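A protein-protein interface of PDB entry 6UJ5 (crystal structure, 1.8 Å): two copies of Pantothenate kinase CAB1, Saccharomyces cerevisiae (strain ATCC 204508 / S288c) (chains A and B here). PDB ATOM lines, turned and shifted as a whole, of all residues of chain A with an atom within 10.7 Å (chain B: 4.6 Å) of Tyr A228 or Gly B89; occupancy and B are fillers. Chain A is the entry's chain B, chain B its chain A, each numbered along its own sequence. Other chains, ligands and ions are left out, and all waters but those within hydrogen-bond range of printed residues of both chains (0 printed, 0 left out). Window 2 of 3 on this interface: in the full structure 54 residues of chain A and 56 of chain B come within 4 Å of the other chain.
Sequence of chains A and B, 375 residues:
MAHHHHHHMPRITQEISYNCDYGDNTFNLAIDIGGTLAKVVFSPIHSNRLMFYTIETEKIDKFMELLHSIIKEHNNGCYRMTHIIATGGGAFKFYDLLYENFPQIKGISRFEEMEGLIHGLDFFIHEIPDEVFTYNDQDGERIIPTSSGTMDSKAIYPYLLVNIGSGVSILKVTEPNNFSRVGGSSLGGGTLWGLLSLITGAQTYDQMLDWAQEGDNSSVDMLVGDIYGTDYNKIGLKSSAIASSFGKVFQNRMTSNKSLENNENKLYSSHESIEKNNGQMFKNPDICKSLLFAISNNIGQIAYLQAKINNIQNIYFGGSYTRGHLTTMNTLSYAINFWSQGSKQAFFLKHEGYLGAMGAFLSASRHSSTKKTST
No position is printed for both chains. Of the 8 pairs that touch across the chains among the printed residues, none has its exchanged pair printed and touching as well.
The backbone NH (N) of Leu A223 is in hydrogen-bond range of the side-chain carboxylate (OD2) of Asp A226, 2.8 Å away. The backbone carbonyl oxygen of Ile B33 lies within hydrogen-bond range of the backbone NH of Gly B90 (2.9 Å). The backbone NH (N) of Gly A225 lies within hydrogen-bond range of the backbone carbonyl oxygen (O) of Ser A239 (2.9 Å). The backbone carbonyl oxygen (O) of Ile B33 is in hydrogen-bond range of the backbone NH (N) of Gly B89 (3.4 Å).
OE1 of Glu B113 lies within hydrogen-bond range of OH of Tyr A228, at 2.7 Å. The side-chain amino group (NZ) of Lys B93 sits at hydrogen-bond distance from the backbone carbonyl oxygen (O) of Asp A226, at 3.4 Å.
Hydrophobic or aromatic side chains of chain A within 4 Å of the printed part of chain B: Ile A227 and Tyr A228. Among the printed residues, 8 pairs touch across the chains. Among the printed residues, no Asp or Glu carboxylate lies within 4 Å of a Lys or Arg side-chain nitrogen of the other chain.
Among the printed residues, pairs that only touch across the chains: Tyr A228 with Gly B89, Ile A227 with Gly B89, Ile A227 with Lys B93, Gly A225 with Lys B93, Ile A227 with Gly B90 and Gly A229 with Lys B93.
Printed residues of chain B within 4 Å of Gly A225: Lys B93. Of the printed residues of chain B, Ile A227 touches Gly B89, Gly B90 and Lys B93. Of the printed residues of chain B, Tyr A228 touches Gly B89 and Glu B113. Of the printed residues of chain B, Gly A229 touches Lys B93 (3.9 Å). Leu A237 touches none of the printed residues of chain B. Of chain A, only Ile A227 (3.5 Å) and Tyr A228 (3.3 Å) come within 4 Å of Gly B89. Of chain A, only Ile A227 comes within 4 Å of Gly B90. Of the printed residues of chain A, Lys B93 touches Gly A225 (3.6 Å), Asp A226 (3.4 Å), Ile A227 (3.5 Å) and Gly A229 (3.9 Å). Of the printed residues of chain A, Glu B113 touches Tyr A228.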
ATOM      1  N   MET A 222      17.704  -3.953 -23.365  1.00  0.00           N
ATOM      2  CA  MET A 222      16.271  -4.226 -23.371  1.00  0.00           C
ATOM      3  C   MET A 222      15.610  -3.300 -22.361  1.00  0.00           C
ATOM      4  O   MET A 222      15.969  -3.319 -21.173  1.00  0.00           O
ATOM      5  CB  MET A 222      15.985  -5.685 -23.019  1.00  0.00           C
ATOM      6  CG  MET A 222      16.308  -6.671 -24.124  1.00  0.00           C
ATOM      7  SD  MET A 222      15.120  -6.587 -25.475  1.00  0.00           S
ATOM      8  CE  MET A 222      13.662  -7.248 -24.678  1.00  0.00           C
ATOM      9  N   LEU A 223      14.682  -2.476 -22.829  1.00  0.00           N
ATOM     10  CA  LEU A 223      13.978  -1.571 -21.939  1.00  0.00           C
ATOM     11  C   LEU A 223      12.707  -2.242 -21.435  1.00  0.00           C
ATOM     12  O   LEU A 223      12.225  -3.221 -22.009  1.00  0.00           O
ATOM     13  CB  LEU A 223      13.629  -0.260 -22.649  1.00  0.00           C
ATOM     14  CG  LEU A 223      14.772   0.429 -23.399  1.00  0.00           C
ATOM     15  CD1 LEU A 223      14.318   1.768 -23.959  1.00  0.00           C
ATOM     16  CD2 LEU A 223      15.993   0.602 -22.484  1.00  0.00           C
ATOM     17  N   VAL A 224      12.168  -1.699 -20.343  1.00  0.00           N
ATOM     18  CA  VAL A 224      10.919  -2.231 -19.810  1.00  0.00           C
ATOM     19  C   VAL A 224       9.855  -2.261 -20.901  1.00  0.00           C
ATOM     20  O   VAL A 224       9.145  -3.261 -21.068  1.00  0.00           O
ATOM     21  CB  VAL A 224      10.481  -1.408 -18.584  1.00  0.00           C
ATOM     22  CG1 VAL A 224       9.044  -1.740 -18.199  1.00  0.00           C
ATOM     23  CG2 VAL A 224      11.425  -1.679 -17.428  1.00  0.00           C
ATOM     24  N   GLY A 225       9.771  -1.191 -21.699  1.00  0.00           N
ATOM     25  CA  GLY A 225       8.819  -1.162 -22.795  1.00  0.00           C
ATOM     26  C   GLY A 225       9.044  -2.249 -23.827  1.00  0.00           C
ATOM     27  O   GLY A 225       8.095  -2.690 -24.480  1.00  0.00           O
ATOM     28  N   ASP A 226      10.293  -2.686 -24.006  1.00  0.00           N
ATOM     29  CA  ASP A 226      10.559  -3.794 -24.920  1.00  0.00           C
ATOM     30  C   ASP A 226       9.914  -5.083 -24.426  1.00  0.00           C
ATOM     31  O   ASP A 226       9.403  -5.873 -25.226  1.00  0.00           O
ATOM     32  CB  ASP A 226      12.065  -4.007 -25.096  1.00  0.00           C
ATOM     33  CG  ASP A 226      12.735  -2.877 -25.859  1.00  0.00           C
ATOM     34  OD1 ASP A 226      12.127  -2.337 -26.806  1.00  0.00           O
ATOM     35  OD2 ASP A 226      13.880  -2.535 -25.507  1.00  0.00           O
ATOM     36  N   ILE A 227       9.942  -5.318 -23.119  1.00  0.00           N
ATOM     37  CA  ILE A 227       9.414  -6.556 -22.554  1.00  0.00           C
ATOM     38  C   ILE A 227       7.924  -6.450 -22.264  1.00  0.00           C
ATOM     39  O   ILE A 227       7.138  -7.305 -22.687  1.00  0.00           O
ATOM     40  CB  ILE A 227      10.207  -6.930 -21.287  1.00  0.00           C
ATOM     41  CG1 ILE A 227      11.680  -7.129 -21.635  1.00  0.00           C
ATOM     42  CG2 ILE A 227       9.626  -8.177 -20.639  1.00  0.00           C
ATOM     43  CD1 ILE A 227      12.576  -7.258 -20.433  1.00  0.00           C
ATOM     44  N   TYR A 228       7.511  -5.404 -21.547  1.00  0.00           N
ATOM     45  CA  TYR A 228       6.149  -5.293 -21.028  1.00  0.00           C
ATOM     46  C   TYR A 228       5.222  -4.464 -21.908  1.00  0.00           C
ATOM     47  O   TYR A 228       4.024  -4.392 -21.620  1.00  0.00           O
ATOM     48  CB  TYR A 228       6.173  -4.698 -19.613  1.00  0.00           C
ATOM     49  CG  TYR A 228       6.947  -5.537 -18.626  1.00  0.00           C
ATOM     50  CD1 TYR A 228       8.318  -5.384 -18.487  1.00  0.00           C
ATOM     51  CD2 TYR A 228       6.309  -6.489 -17.840  1.00  0.00           C
ATOM     52  CE1 TYR A 228       9.040  -6.158 -17.592  1.00  0.00           C
ATOM     53  CE2 TYR A 228       7.019  -7.264 -16.939  1.00  0.00           C
ATOM     54  CZ  TYR A 228       8.385  -7.100 -16.818  1.00  0.00           C
ATOM     55  OH  TYR A 228       9.108  -7.872 -15.929  1.00  0.00           O
ATOM     56  N   GLY A 229       5.736  -3.842 -22.964  1.00  0.00           N
ATOM     57  CA  GLY A 229       4.912  -2.922 -23.729  1.00  0.00           C
ATOM     58  C   GLY A 229       4.548  -1.701 -22.904  1.00  0.00           C
ATOM     59  O   GLY A 229       5.352  -1.180 -22.125  1.00  0.00           O
ATOM     60  N   THR A 230       3.308  -1.243 -23.066  1.00  0.00           N
ATOM     61  CA  THR A 230       2.819  -0.067 -22.352  1.00  0.00           C
ATOM     62  C   THR A 230       1.391  -0.272 -21.850  1.00  0.00           C
ATOM     63  O   THR A 230       1.127  -0.194 -20.649  1.00  0.00           O
ATOM     64  CB  THR A 230       2.865   1.186 -23.246  1.00  0.00           C
ATOM     65  OG1 THR A 230       2.377   0.859 -24.553  1.00  0.00           O
ATOM     66  CG2 THR A 230       4.287   1.714 -23.356  1.00  0.00           C
ATOM     67  N   LEU A 237       8.262   0.818 -12.617  1.00  0.00           N
ATOM     68  CA  LEU A 237       9.251   1.182 -13.626  1.00  0.00           C
ATOM     69  C   LEU A 237       8.616   1.755 -14.900  1.00  0.00           C
ATOM     70  O   LEU A 237       7.675   1.181 -15.451  1.00  0.00           O
ATOM     71  CB  LEU A 237      10.114  -0.031 -13.970  1.00  0.00           C
ATOM     72  CG  LEU A 237      11.057  -0.479 -12.856  1.00  0.00           C
ATOM     73  CD1 LEU A 237      11.949  -1.632 -13.314  1.00  0.00           C
ATOM     74  CD2 LEU A 237      11.902   0.699 -12.392  1.00  0.00           C
ATOM     75  N   LYS A 238       9.137   2.894 -15.357  1.00  0.00           N
ATOM     76  CA  LYS A 238       8.679   3.506 -16.593  1.00  0.00           C
ATOM     77  C   LYS A 238       9.142   2.686 -17.798  1.00  0.00           C
ATOM     78  O   LYS A 238      10.044   1.854 -17.703  1.00  0.00           O
ATOM     79  CB  LYS A 238       9.193   4.942 -16.699  1.00  0.00           C
ATOM     80  N   SER A 239       8.494   2.921 -18.941  1.00  0.00           N
ATOM     81  CA  SER A 239       8.813   2.160 -20.149  1.00  0.00           C
ATOM     82  C   SER A 239      10.274   2.324 -20.543  1.00  0.00           C
ATOM     83  O   SER A 239      10.893   1.386 -21.059  1.00  0.00           O
ATOM     84  CB  SER A 239       7.916   2.596 -21.305  1.00  0.00           C
ATOM     85  OG  SER A 239       6.609   2.078 -21.165  1.00  0.00           O
ATOM     86  N   SER A 240      10.837   3.515 -20.334  1.00  0.00           N
ATOM     87  CA  SER A 240      12.201   3.793 -20.768  1.00  0.00           C
ATOM     88  C   SER A 240      13.255   3.256 -19.809  1.00  0.00           C
ATOM     89  O   SER A 240      14.446   3.298 -20.140  1.00  0.00           O
ATOM     90  CB  SER A 240      12.396   5.297 -20.940  1.00  0.00           C
ATOM     91  OG  SER A 240      12.183   5.953 -19.707  1.00  0.00           O
ATOM     92  N   ALA A 241      12.857   2.772 -18.635  1.00  0.00           N
ATOM     93  CA  ALA A 241      13.808   2.186 -17.705  1.00  0.00           C
ATOM     94  C   ALA A 241      14.473   0.963 -18.328  1.00  0.00           C
ATOM     95  O   ALA A 241      13.915   0.300 -19.203  1.00  0.00           O
ATOM     96  CB  ALA A 241      13.114   1.793 -16.401  1.00  0.00           C
ATOM     97  N   ILE A 242      15.678   0.661 -17.863  1.00  0.00           N
ATOM     98  CA  ILE A 242      16.457  -0.441 -18.410  1.00  0.00           C
ATOM     99  C   ILE A 242      16.059  -1.722 -17.694  1.00  0.00           C
ATOM    100  O   ILE A 242      16.156  -1.815 -16.468  1.00  0.00           O
ATOM    101  CB  ILE A 242      17.963  -0.174 -18.269  1.00  0.00           C
ATOM    102  CG1 ILE A 242      18.322   1.151 -18.934  1.00  0.00           C
ATOM    103  CG2 ILE A 242      18.772  -1.315 -18.870  1.00  0.00           C
ATOM    104  CD1 ILE A 242      19.786   1.541 -18.753  1.00  0.00           C
ATOM    105  N   ALA A 243      15.618  -2.716 -18.456  1.00  0.00           N
ATOM    106  CA  ALA A 243      15.301  -4.014 -17.877  1.00  0.00           C
ATOM    107  C   ALA A 243      16.474  -4.977 -17.960  1.00  0.00           C
ATOM    108  O   ALA A 243      16.709  -5.751 -17.029  1.00  0.00           O
ATOM    109  CB  ALA A 243      14.082  -4.625 -18.576  1.00  0.00           C
ATOM    110  N   SER A 244      17.232  -4.943 -19.052  1.00  0.00           N
ATOM    111  CA  SER A 244      18.351  -5.861 -19.227  1.00  0.00           C
ATOM    112  C   SER A 244      19.468  -5.124 -19.955  1.00  0.00           C
ATOM    113  O   SER A 244      19.374  -4.894 -21.166  1.00  0.00           O
ATOM    114  CB  SER A 244      17.919  -7.101 -20.006  1.00  0.00           C
ATOM    115  OG  SER A 244      18.974  -8.046 -20.069  1.00  0.00           O
ATOM    116  N   ILE B  33       6.635 -15.898 -21.661  1.00  0.00           N
ATOM    117  CA  ILE B  33       7.222 -15.134 -22.745  1.00  0.00           C
ATOM    118  C   ILE B  33       8.135 -14.108 -22.094  1.00  0.00           C
ATOM    119  O   ILE B  33       7.672 -13.087 -21.579  1.00  0.00           O
ATOM    120  CB  ILE B  33       6.156 -14.475 -23.617  1.00  0.00           C
ATOM    121  CG1 ILE B  33       5.177 -15.530 -24.123  1.00  0.00           C
ATOM    122  CG2 ILE B  33       6.812 -13.781 -24.789  1.00  0.00           C
ATOM    123  CD1 ILE B  33       4.045 -14.955 -24.950  1.00  0.00           C
ATOM    124  N   THR B  87       2.086 -16.076 -19.762  1.00  0.00           N
ATOM    125  CA  THR B  87       2.647 -15.472 -18.553  1.00  0.00           C
ATOM    126  C   THR B  87       4.002 -14.880 -18.930  1.00  0.00           C
ATOM    127  O   THR B  87       4.334 -14.735 -20.112  1.00  0.00           O
ATOM    128  CB  THR B  87       2.734 -16.482 -17.395  1.00  0.00           C
ATOM    129  OG1 THR B  87       3.017 -15.791 -16.166  1.00  0.00           O
ATOM    130  CG2 THR B  87       3.828 -17.524 -17.658  1.00  0.00           C
ATOM    131  N   GLY B  88       4.793 -14.519 -17.927  1.00  0.00           N
ATOM    132  CA  GLY B  88       6.045 -13.845 -18.189  1.00  0.00           C
ATOM    133  C   GLY B  88       5.816 -12.374 -18.419  1.00  0.00           C
ATOM    134  O   GLY B  88       4.689 -11.876 -18.425  1.00  0.00           O
ATOM    135  N   GLY B  89       6.919 -11.651 -18.600  1.00  0.00           N
ATOM    136  CA  GLY B  89       6.810 -10.221 -18.781  1.00  0.00           C
ATOM    137  C   GLY B  89       6.015  -9.848 -20.015  1.00  0.00           C
ATOM    138  O   GLY B  89       5.365  -8.799 -20.047  1.00  0.00           O
ATOM    139  N   GLY B  90       6.040 -10.698 -21.033  1.00  0.00           N
ATOM    140  CA  GLY B  90       5.350 -10.433 -22.279  1.00  0.00           C
ATOM    141  C   GLY B  90       3.912 -10.904 -22.369  1.00  0.00           C
ATOM    142  O   GLY B  90       3.312 -10.780 -23.441  1.00  0.00           O
ATOM    143  N   ALA B  91       3.331 -11.405 -21.276  1.00  0.00           N
ATOM    144  CA  ALA B  91       2.006 -12.026 -21.331  1.00  0.00           C
ATOM    145  C   ALA B  91       0.948 -11.065 -21.864  1.00  0.00           C
ATOM    146  O   ALA B  91       0.227 -11.379 -22.818  1.00  0.00           O
ATOM    147  CB  ALA B  91       1.611 -12.525 -19.945  1.00  0.00           C
ATOM    148  N   LYS B  93       1.425  -8.147 -23.297  1.00  0.00           N
ATOM    149  CA  LYS B  93       1.873  -7.551 -24.552  1.00  0.00           C
ATOM    150  C   LYS B  93       1.473  -8.399 -25.752  1.00  0.00           C
ATOM    151  O   LYS B  93       0.952  -7.878 -26.744  1.00  0.00           O
ATOM    152  CB  LYS B  93       3.394  -7.364 -24.509  1.00  0.00           C
ATOM    153  CG  LYS B  93       4.035  -6.908 -25.817  1.00  0.00           C
ATOM    154  CD  LYS B  93       5.530  -7.236 -25.817  1.00  0.00           C
ATOM    155  CE  LYS B  93       6.293  -6.524 -26.930  1.00  0.00           C
ATOM    156  NZ  LYS B  93       6.464  -5.065 -26.645  1.00  0.00           N
ATOM    157  N   GLU B 113       3.090 -11.999 -14.191  1.00  0.00           N
ATOM    158  CA  GLU B 113       4.412 -12.612 -14.139  1.00  0.00           C
ATOM    159  C   GLU B 113       4.801 -12.993 -12.716  1.00  0.00           C
ATOM    160  O   GLU B 113       5.205 -14.131 -12.450  1.00  0.00           O
ATOM    161  CB  GLU B 113       5.446 -11.654 -14.736  1.00  0.00           C
ATOM    162  CG  GLU B 113       6.874 -12.176 -14.705  1.00  0.00           C
ATOM    163  CD  GLU B 113       7.894 -11.118 -15.088  1.00  0.00           C
ATOM    164  OE1 GLU B 113       7.551  -9.917 -15.072  1.00  0.00           O
ATOM    165  OE2 GLU B 113       9.039 -11.492 -15.407  1.00  0.00           O
ATOM    166  N   MET B 114       4.711 -12.045 -11.786  1.00  0.00           N
ATOM    167  CA  MET B 114       5.182 -12.338 -10.440  1.00  0.00           C
ATOM    168  C   MET B 114       4.321 -13.415  -9.781  1.00  0.00           C
ATOM    169  O   MET B 114       4.859 -14.343  -9.164  1.00  0.00           O
ATOM    170  CB  MET B 114       5.234 -11.051  -9.605  1.00  0.00           C
ATOM    171  CG  MET B 114       5.998  -9.889 -10.286  1.00  0.00           C
ATOM    172  SD  MET B 114       7.710 -10.209 -10.826  1.00  0.00           S
ATOM    173  CE  MET B 114       8.052  -8.725 -11.770  1.00  0.00           C
